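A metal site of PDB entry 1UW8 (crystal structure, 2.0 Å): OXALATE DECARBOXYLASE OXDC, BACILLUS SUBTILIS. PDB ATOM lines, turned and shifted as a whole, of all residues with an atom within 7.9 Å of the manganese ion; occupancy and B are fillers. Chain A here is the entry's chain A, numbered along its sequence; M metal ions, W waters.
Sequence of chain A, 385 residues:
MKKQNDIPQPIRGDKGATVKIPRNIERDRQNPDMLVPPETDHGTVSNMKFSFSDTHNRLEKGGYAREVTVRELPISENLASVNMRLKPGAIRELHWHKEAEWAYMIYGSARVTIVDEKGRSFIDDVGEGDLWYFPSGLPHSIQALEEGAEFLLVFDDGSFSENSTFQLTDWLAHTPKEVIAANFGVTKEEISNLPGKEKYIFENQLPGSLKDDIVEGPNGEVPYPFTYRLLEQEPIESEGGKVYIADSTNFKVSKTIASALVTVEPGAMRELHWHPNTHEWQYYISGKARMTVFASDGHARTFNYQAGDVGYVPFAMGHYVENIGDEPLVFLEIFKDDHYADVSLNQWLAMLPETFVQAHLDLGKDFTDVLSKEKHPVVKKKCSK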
ATOM      1  N   MET A  84      19.495  22.767  -3.494  1.00  0.00           N
ATOM      2  CA  MET A  84      20.398  23.012  -4.615  1.00  0.00           C
ATOM      3  C   MET A  84      21.785  23.444  -4.110  1.00  0.00           C
ATOM      4  O   MET A  84      21.910  24.239  -3.168  1.00  0.00           O
ATOM      5  CB  MET A  84      19.841  24.100  -5.543  1.00  0.00           C
ATOM      6  CG  MET A  84      20.713  24.351  -6.791  1.00  0.00           C
ATOM      7  SD  MET A  84      19.899  25.299  -8.072  1.00  0.00           S
ATOM      8  CE  MET A  84      18.785  24.031  -8.746  1.00  0.00           C
ATOM      9  N   ARG A  92      23.355  28.466 -12.154  1.00  0.00           N
ATOM     10  CA  ARG A  92      22.011  27.948 -12.430  1.00  0.00           C
ATOM     11  C   ARG A  92      21.410  28.833 -13.513  1.00  0.00           C
ATOM     12  O   ARG A  92      21.169  30.035 -13.327  1.00  0.00           O
ATOM     13  CB  ARG A  92      21.155  27.950 -11.157  1.00  0.00           C
ATOM     14  CG  ARG A  92      19.735  27.460 -11.370  1.00  0.00           C
ATOM     15  CD  ARG A  92      19.596  26.004 -11.800  1.00  0.00           C
ATOM     16  NE  ARG A  92      18.182  25.671 -12.021  1.00  0.00           N
ATOM     17  CZ  ARG A  92      17.559  25.649 -13.220  1.00  0.00           C
ATOM     18  NH1 ARG A  92      18.237  25.908 -14.339  1.00  0.00           N
ATOM     19  NH2 ARG A  92      16.265  25.378 -13.307  1.00  0.00           N
ATOM     20  N   GLU A  93      21.259  28.202 -14.673  1.00  0.00           N
ATOM     21  CA  GLU A  93      20.920  28.836 -15.926  1.00  0.00           C
ATOM     22  C   GLU A  93      19.702  29.734 -15.811  1.00  0.00           C
ATOM     23  O   GLU A  93      18.701  29.378 -15.175  1.00  0.00           O
ATOM     24  CB  GLU A  93      20.618  27.746 -16.989  1.00  0.00           C
ATOM     25  CG  GLU A  93      20.251  28.313 -18.331  1.00  0.00           C
ATOM     26  CD  GLU A  93      19.994  27.326 -19.457  1.00  0.00           C
ATOM     27  OE1 GLU A  93      20.181  26.115 -19.332  1.00  0.00           O
ATOM     28  OE2 GLU A  93      19.622  27.814 -20.527  1.00  0.00           O
ATOM     29  N   LEU A  94      19.811  30.896 -16.424  1.00  0.00           N
ATOM     30  CA  LEU A  94      18.703  31.801 -16.656  1.00  0.00           C
ATOM     31  C   LEU A  94      17.407  31.074 -17.041  1.00  0.00           C
ATOM     32  O   LEU A  94      17.374  30.343 -18.045  1.00  0.00           O
ATOM     33  CB  LEU A  94      19.100  32.784 -17.771  1.00  0.00           C
ATOM     34  CG  LEU A  94      20.017  33.935 -17.335  1.00  0.00           C
ATOM     35  CD1 LEU A  94      20.687  34.597 -18.553  1.00  0.00           C
ATOM     36  CD2 LEU A  94      19.240  34.981 -16.523  1.00  0.00           C
ATOM     37  N   HIS A  95      16.360  31.282 -16.253  1.00  0.00           N
ATOM     38  CA  HIS A  95      15.147  30.506 -16.377  1.00  0.00           C
ATOM     39  C   HIS A  95      13.959  31.209 -15.723  1.00  0.00           C
ATOM     40  O   HIS A  95      14.091  32.249 -15.050  1.00  0.00           O
ATOM     41  CB  HIS A  95      15.338  29.080 -15.780  1.00  0.00           C
ATOM     42  CG  HIS A  95      15.416  29.041 -14.280  1.00  0.00           C
ATOM     43  ND1 HIS A  95      16.612  29.132 -13.589  1.00  0.00           N
ATOM     44  CD2 HIS A  95      14.444  28.936 -13.336  1.00  0.00           C
ATOM     45  CE1 HIS A  95      16.368  29.079 -12.283  1.00  0.00           C
ATOM     46  NE2 HIS A  95      15.063  28.971 -12.102  1.00  0.00           N
ATOM     47  N   TRP A  96      12.785  30.640 -15.946  1.00  0.00           N
ATOM     48  CA  TRP A  96      11.591  31.125 -15.293  1.00  0.00           C
ATOM     49  C   TRP A  96      10.629  29.954 -15.092  1.00  0.00           C
ATOM     50  O   TRP A  96      10.865  28.842 -15.589  1.00  0.00           O
ATOM     51  CB  TRP A  96      10.946  32.284 -16.076  1.00  0.00           C
ATOM     52  CG  TRP A  96      10.229  31.903 -17.366  1.00  0.00           C
ATOM     53  CD1 TRP A  96       8.871  31.727 -17.539  1.00  0.00           C
ATOM     54  CD2 TRP A  96      10.819  31.676 -18.651  1.00  0.00           C
ATOM     55  NE1 TRP A  96       8.604  31.389 -18.835  1.00  0.00           N
ATOM     56  CE2 TRP A  96       9.776  31.373 -19.550  1.00  0.00           C
ATOM     57  CE3 TRP A  96      12.127  31.715 -19.139  1.00  0.00           C
ATOM     58  CZ2 TRP A  96      10.001  31.071 -20.887  1.00  0.00           C
ATOM     59  CZ3 TRP A  96      12.350  31.404 -20.479  1.00  0.00           C
ATOM     60  CH2 TRP A  96      11.289  31.092 -21.332  1.00  0.00           C
ATOM     61  N   HIS A  97       9.607  30.177 -14.298  1.00  0.00           N
ATOM     62  CA  HIS A  97       8.549  29.195 -14.080  1.00  0.00           C
ATOM     63  C   HIS A  97       7.247  29.866 -13.635  1.00  0.00           C
ATOM     64  O   HIS A  97       7.231  31.036 -13.215  1.00  0.00           O
ATOM     65  CB  HIS A  97       8.975  28.117 -13.066  1.00  0.00           C
ATOM     66  CG  HIS A  97       9.975  28.585 -12.048  1.00  0.00           C
ATOM     67  ND1 HIS A  97       9.673  29.516 -11.083  1.00  0.00           N
ATOM     68  CD2 HIS A  97      11.274  28.255 -11.859  1.00  0.00           C
ATOM     69  CE1 HIS A  97      10.758  29.765 -10.368  1.00  0.00           C
ATOM     70  NE2 HIS A  97      11.749  29.024 -10.831  1.00  0.00           N
ATOM     71  N   GLU A  99       5.547  29.159 -10.893  1.00  0.00           N
ATOM     72  CA  GLU A  99       5.539  29.278  -9.469  1.00  0.00           C
ATOM     73  C   GLU A  99       6.400  30.476  -9.015  1.00  0.00           C
ATOM     74  O   GLU A  99       7.430  30.793  -9.638  1.00  0.00           O
ATOM     75  CB  GLU A  99       6.102  27.993  -8.878  1.00  0.00           C
ATOM     76  CG  GLU A  99       5.219  26.777  -9.122  1.00  0.00           C
ATOM     77  CD  GLU A  99       5.363  26.134 -10.503  1.00  0.00           C
ATOM     78  OE1 GLU A  99       6.296  26.418 -11.265  1.00  0.00           O
ATOM     79  OE2 GLU A  99       4.484  25.337 -10.837  1.00  0.00           O
ATOM     80  N   ALA A 100       5.975  31.092  -7.925  1.00  0.00           N
ATOM     81  CA  ALA A 100       6.849  31.966  -7.153  1.00  0.00           C
ATOM     82  C   ALA A 100       7.880  31.093  -6.427  1.00  0.00           C
ATOM     83  O   ALA A 100       7.617  29.940  -6.077  1.00  0.00           O
ATOM     84  CB  ALA A 100       6.040  32.825  -6.161  1.00  0.00           C
ATOM     85  N   GLU A 101       9.060  31.664  -6.212  1.00  0.00           N
ATOM     86  CA  GLU A 101      10.181  31.001  -5.589  1.00  0.00           C
ATOM     87  C   GLU A 101      10.679  31.785  -4.388  1.00  0.00           C
ATOM     88  O   GLU A 101      10.928  32.972  -4.491  1.00  0.00           O
ATOM     89  CB  GLU A 101      11.309  30.835  -6.593  1.00  0.00           C
ATOM     90  CG  GLU A 101      12.648  30.382  -6.027  1.00  0.00           C
ATOM     91  CD  GLU A 101      13.637  30.178  -7.162  1.00  0.00           C
ATOM     92  OE1 GLU A 101      13.193  29.789  -8.267  1.00  0.00           O
ATOM     93  OE2 GLU A 101      14.839  30.399  -6.985  1.00  0.00           O
ATOM     94  N   TRP A 102      10.825  31.090  -3.267  1.00  0.00           N
ATOM     95  CA  TRP A 102      11.426  31.659  -2.069  1.00  0.00           C
ATOM     96  C   TRP A 102      12.671  30.861  -1.770  1.00  0.00           C
ATOM     97  O   TRP A 102      12.697  29.657  -2.020  1.00  0.00           O
ATOM     98  CB  TRP A 102      10.413  31.568  -0.947  1.00  0.00           C
ATOM     99  CG  TRP A 102      10.832  32.079   0.389  1.00  0.00           C
ATOM    100  CD1 TRP A 102      10.518  33.279   0.922  1.00  0.00           C
ATOM    101  CD2 TRP A 102      11.564  31.369   1.403  1.00  0.00           C
ATOM    102  NE1 TRP A 102      11.020  33.387   2.189  1.00  0.00           N
ATOM    103  CE2 TRP A 102      11.673  32.239   2.513  1.00  0.00           C
ATOM    104  CE3 TRP A 102      12.137  30.109   1.479  1.00  0.00           C
ATOM    105  CZ2 TRP A 102      12.346  31.887   3.675  1.00  0.00           C
ATOM    106  CZ3 TRP A 102      12.821  29.747   2.635  1.00  0.00           C
ATOM    107  CH2 TRP A 102      12.928  30.643   3.724  1.00  0.00           C
ATOM    108  N   TRP A 132      15.885  35.139  -0.831  1.00  0.00           N
ATOM    109  CA  TRP A 132      15.296  35.810  -1.987  1.00  0.00           C
ATOM    110  C   TRP A 132      13.860  35.371  -2.226  1.00  0.00           C
ATOM    111  O   TRP A 132      13.417  34.376  -1.692  1.00  0.00           O
ATOM    112  CB  TRP A 132      16.151  35.702  -3.252  1.00  0.00           C
ATOM    113  CG  TRP A 132      16.307  34.345  -3.886  1.00  0.00           C
ATOM    114  CD1 TRP A 132      15.350  33.644  -4.589  1.00  0.00           C
ATOM    115  CD2 TRP A 132      17.493  33.551  -3.934  1.00  0.00           C
ATOM    116  NE1 TRP A 132      15.874  32.454  -5.047  1.00  0.00           N
ATOM    117  CE2 TRP A 132      17.187  32.376  -4.666  1.00  0.00           C
ATOM    118  CE3 TRP A 132      18.787  33.693  -3.425  1.00  0.00           C
ATOM    119  CZ2 TRP A 132      18.112  31.376  -4.888  1.00  0.00           C
ATOM    120  CZ3 TRP A 132      19.698  32.717  -3.652  1.00  0.00           C
ATOM    121  CH2 TRP A 132      19.362  31.549  -4.390  1.00  0.00           C
ATOM    122  N   PHE A 134      11.343  35.486  -5.851  1.00  0.00           N
ATOM    123  CA  PHE A 134      11.109  35.815  -7.239  1.00  0.00           C
ATOM    124  C   PHE A 134       9.633  35.601  -7.517  1.00  0.00           C
ATOM    125  O   PHE A 134       9.163  34.489  -7.448  1.00  0.00           O
ATOM    126  CB  PHE A 134      11.952  34.927  -8.141  1.00  0.00           C
ATOM    127  CG  PHE A 134      13.432  35.000  -7.883  1.00  0.00           C
ATOM    128  CD1 PHE A 134      14.020  36.186  -7.459  1.00  0.00           C
ATOM    129  CD2 PHE A 134      14.230  33.886  -8.071  1.00  0.00           C
ATOM    130  CE1 PHE A 134      15.379  36.257  -7.242  1.00  0.00           C
ATOM    131  CE2 PHE A 134      15.601  33.945  -7.860  1.00  0.00           C
ATOM    132  CZ  PHE A 134      16.172  35.137  -7.446  1.00  0.00           C
ATOM    133  N   LEU A 138       8.779  35.637 -13.358  1.00  0.00           N
ATOM    134  CA  LEU A 138       9.854  36.591 -13.640  1.00  0.00           C
ATOM    135  C   LEU A 138      11.167  35.850 -13.731  1.00  0.00           C
ATOM    136  O   LEU A 138      11.450  34.949 -12.912  1.00  0.00           O
ATOM    137  CB  LEU A 138       9.923  37.699 -12.580  1.00  0.00           C
ATOM    138  CG  LEU A 138       8.696  38.599 -12.469  1.00  0.00           C
ATOM    139  CD1 LEU A 138       8.942  39.713 -11.462  1.00  0.00           C
ATOM    140  CD2 LEU A 138       8.295  39.178 -13.830  1.00  0.00           C
ATOM    141  N   PRO A 139      11.937  36.145 -14.762  1.00  0.00           N
ATOM    142  CA  PRO A 139      13.126  35.351 -15.059  1.00  0.00           C
ATOM    143  C   PRO A 139      14.321  35.710 -14.186  1.00  0.00           C
ATOM    144  O   PRO A 139      14.522  36.895 -13.841  1.00  0.00           O
ATOM    145  CB  PRO A 139      13.411  35.686 -16.511  1.00  0.00           C
ATOM    146  CG  PRO A 139      12.910  37.096 -16.651  1.00  0.00           C
ATOM    147  CD  PRO A 139      11.710  37.199 -15.761  1.00  0.00           C
ATOM    148  N   HIS A 140      15.133  34.701 -13.895  1.00  0.00           N
ATOM    149  CA  HIS A 140      16.168  34.836 -12.907  1.00  0.00           C
ATOM    150  C   HIS A 140      17.292  33.810 -13.113  1.00  0.00           C
ATOM    151  O   HIS A 140      17.183  32.859 -13.901  1.00  0.00           O
ATOM    152  CB  HIS A 140      15.567  34.762 -11.496  1.00  0.00           C
ATOM    153  CG  HIS A 140      14.748  33.515 -11.251  1.00  0.00           C
ATOM    154  ND1 HIS A 140      13.414  33.418 -11.587  1.00  0.00           N
ATOM    155  CD2 HIS A 140      15.092  32.306 -10.739  1.00  0.00           C
ATOM    156  CE1 HIS A 140      12.966  32.211 -11.279  1.00  0.00           C
ATOM    157  NE2 HIS A 140      13.962  31.527 -10.739  1.00  0.00           N
ATOM    158  N   SER A 141      18.369  34.053 -12.368  1.00  0.00           N
ATOM    159  CA  SER A 141      19.577  33.236 -12.382  1.00  0.00           C
ATOM    160  C   SER A 141      20.232  33.248 -10.996  1.00  0.00           C
ATOM    161  O   SER A 141      19.974  34.130 -10.154  1.00  0.00           O
ATOM    162  CB  SER A 141      20.574  33.729 -13.429  1.00  0.00           C
ATOM    163  OG  SER A 141      21.116  34.996 -13.047  1.00  0.00           O
ATOM    164  N   ILE A 142      21.066  32.240 -10.763  1.00  0.00           N
ATOM    165  CA  ILE A 142      21.882  32.153  -9.541  1.00  0.00           C
ATOM    166  C   ILE A 142      23.302  31.787  -9.985  1.00  0.00           C
ATOM    167  O   ILE A 142      23.476  30.912 -10.844  1.00  0.00           O
ATOM    168  CB  ILE A 142      21.382  31.035  -8.608  1.00  0.00           C
ATOM    169  CG1 ILE A 142      19.870  31.056  -8.395  1.00  0.00           C
ATOM    170  CG2 ILE A 142      22.094  31.107  -7.248  1.00  0.00           C
ATOM    171  CD1 ILE A 142      19.307  29.715  -7.858  1.00  0.00           C
ATOM    172  N   LEU A 153      15.228  26.027  -1.706  1.00  0.00           N
ATOM    173  CA  LEU A 153      14.221  26.740  -2.476  1.00  0.00           C
ATOM    174  C   LEU A 153      12.854  26.184  -2.140  1.00  0.00           C
ATOM    175  O   LEU A 153      12.682  24.960  -1.982  1.00  0.00           O
ATOM    176  CB  LEU A 153      14.505  26.563  -3.971  1.00  0.00           C
ATOM    177  CG  LEU A 153      15.884  26.950  -4.518  1.00  0.00           C
ATOM    178  CD1 LEU A 153      16.058  26.531  -5.976  1.00  0.00           C
ATOM    179  CD2 LEU A 153      16.111  28.436  -4.386  1.00  0.00           C
ATOM    180  N   PHE A 155       8.767  26.507  -3.576  1.00  0.00           N
ATOM    181  CA  PHE A 155       7.905  26.914  -4.672  1.00  0.00           C
ATOM    182  C   PHE A 155       6.474  26.776  -4.252  1.00  0.00           C
ATOM    183  O   PHE A 155       6.115  25.788  -3.591  1.00  0.00           O
ATOM    184  CB  PHE A 155       8.170  26.020  -5.881  1.00  0.00           C
ATOM    185  CG  PHE A 155       9.584  26.076  -6.336  1.00  0.00           C
ATOM    186  CD1 PHE A 155      10.520  25.212  -5.790  1.00  0.00           C
ATOM    187  CD2 PHE A 155       9.998  27.072  -7.188  1.00  0.00           C
ATOM    188  CE1 PHE A 155      11.827  25.293  -6.153  1.00  0.00           C
ATOM    189  CE2 PHE A 155      11.334  27.160  -7.556  1.00  0.00           C
ATOM    190  CZ  PHE A 155      12.246  26.253  -7.031  1.00  0.00           C
ATOM    191  N   PHE A 160       5.370  21.238  -8.545  1.00  0.00           N
ATOM    192  CA  PHE A 160       6.583  21.709  -9.196  1.00  0.00           C
ATOM    193  C   PHE A 160       7.627  20.590  -9.396  1.00  0.00           C
ATOM    194  O   PHE A 160       7.745  19.695  -8.538  1.00  0.00           O
ATOM    195  CB  PHE A 160       7.190  22.791  -8.287  1.00  0.00           C
ATOM    196  CG  PHE A 160       8.436  23.408  -8.835  1.00  0.00           C
ATOM    197  CD1 PHE A 160       8.361  24.406  -9.793  1.00  0.00           C
ATOM    198  CD2 PHE A 160       9.675  23.014  -8.394  1.00  0.00           C
ATOM    199  CE1 PHE A 160       9.526  24.995 -10.301  1.00  0.00           C
ATOM    200  CE2 PHE A 160      10.819  23.607  -8.903  1.00  0.00           C
ATOM    201  CZ  PHE A 160      10.734  24.574  -9.860  1.00  0.00           C
ATOM    202  N   GLU A 162      12.007  20.902 -10.472  1.00  0.00           N
ATOM    203  CA  GLU A 162      13.166  21.687 -10.965  1.00  0.00           C
ATOM    204  C   GLU A 162      13.612  21.237 -12.351  1.00  0.00           C
ATOM    205  O   GLU A 162      14.272  22.007 -13.045  1.00  0.00           O
ATOM    206  CB  GLU A 162      14.356  21.658  -9.963  1.00  0.00           C
ATOM    207  CG  GLU A 162      15.471  22.677 -10.198  1.00  0.00           C
ATOM    208  CD  GLU A 162      15.078  24.137  -9.902  1.00  0.00           C
ATOM    209  OE1 GLU A 162      14.096  24.366  -9.153  1.00  0.00           O
ATOM    210  OE2 GLU A 162      15.773  25.073 -10.405  1.00  0.00           O
ATOM    211  N   THR A 165      11.647  23.639 -15.419  1.00  0.00           N
ATOM    212  CA  THR A 165      11.638  25.077 -15.564  1.00  0.00           C
ATOM    213  C   THR A 165      11.809  25.425 -17.039  1.00  0.00           C
ATOM    214  O   THR A 165      12.234  24.584 -17.817  1.00  0.00           O
ATOM    215  CB  THR A 165      12.757  25.739 -14.728  1.00  0.00           C
ATOM    216  OG1 THR A 165      14.022  25.427 -15.286  1.00  0.00           O
ATOM    217  CG2 THR A 165      12.776  25.179 -13.320  1.00  0.00           C
HETATM  218 MN    MN M   1      13.923  29.319 -10.205  1.00  0.00          MN
HETATM  219  O   HOH W   1      16.001  29.468  -9.148  1.00  0.00           O
HETATM  220  O   HOH W   2      13.881  27.018  -9.961  1.00  0.00           O
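The backbone NH (N) of Phe 134 is in hydrogen-bond range of the backbone carbonyl oxygen (O) of Glu 101.
The indole nitrogen of Trp 132 is in hydrogen-bond range of the side-chain carboxylate of Glu 101 (3.0 Å).
O of Glu 93 lies within hydrogen-bond range of ND1 of His 95 (2.6 Å).
The backbone carbonyl oxygen (O) of Leu 138 is in hydrogen-bond range of a ring nitrogen (ND1) of His 140 (2.8 Å).
A ring nitrogen (ND1) of His 97 lies within hydrogen-bond range of the backbone carbonyl oxygen (O) of Glu 99, 3.0 Å away.
Of the 23 residues printed, 4 come within 4 Å of the manganese ion.
OE1 of Glu 101 is bound to the manganese ion (2.1 Å).
The manganese ion is bound by NE2 of His 95 (2.2 Å).
NE2 of His 140 binds the manganese ion (2.3 Å).
NE2 of His 97 is bound to the manganese ion, at 2.3 Å.
The manganese ion is bound by water W2, 2.3 Å away.
The manganese ion is bound by water W1 (2.3 Å).
The manganese ion has six donor atoms within binding distance.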
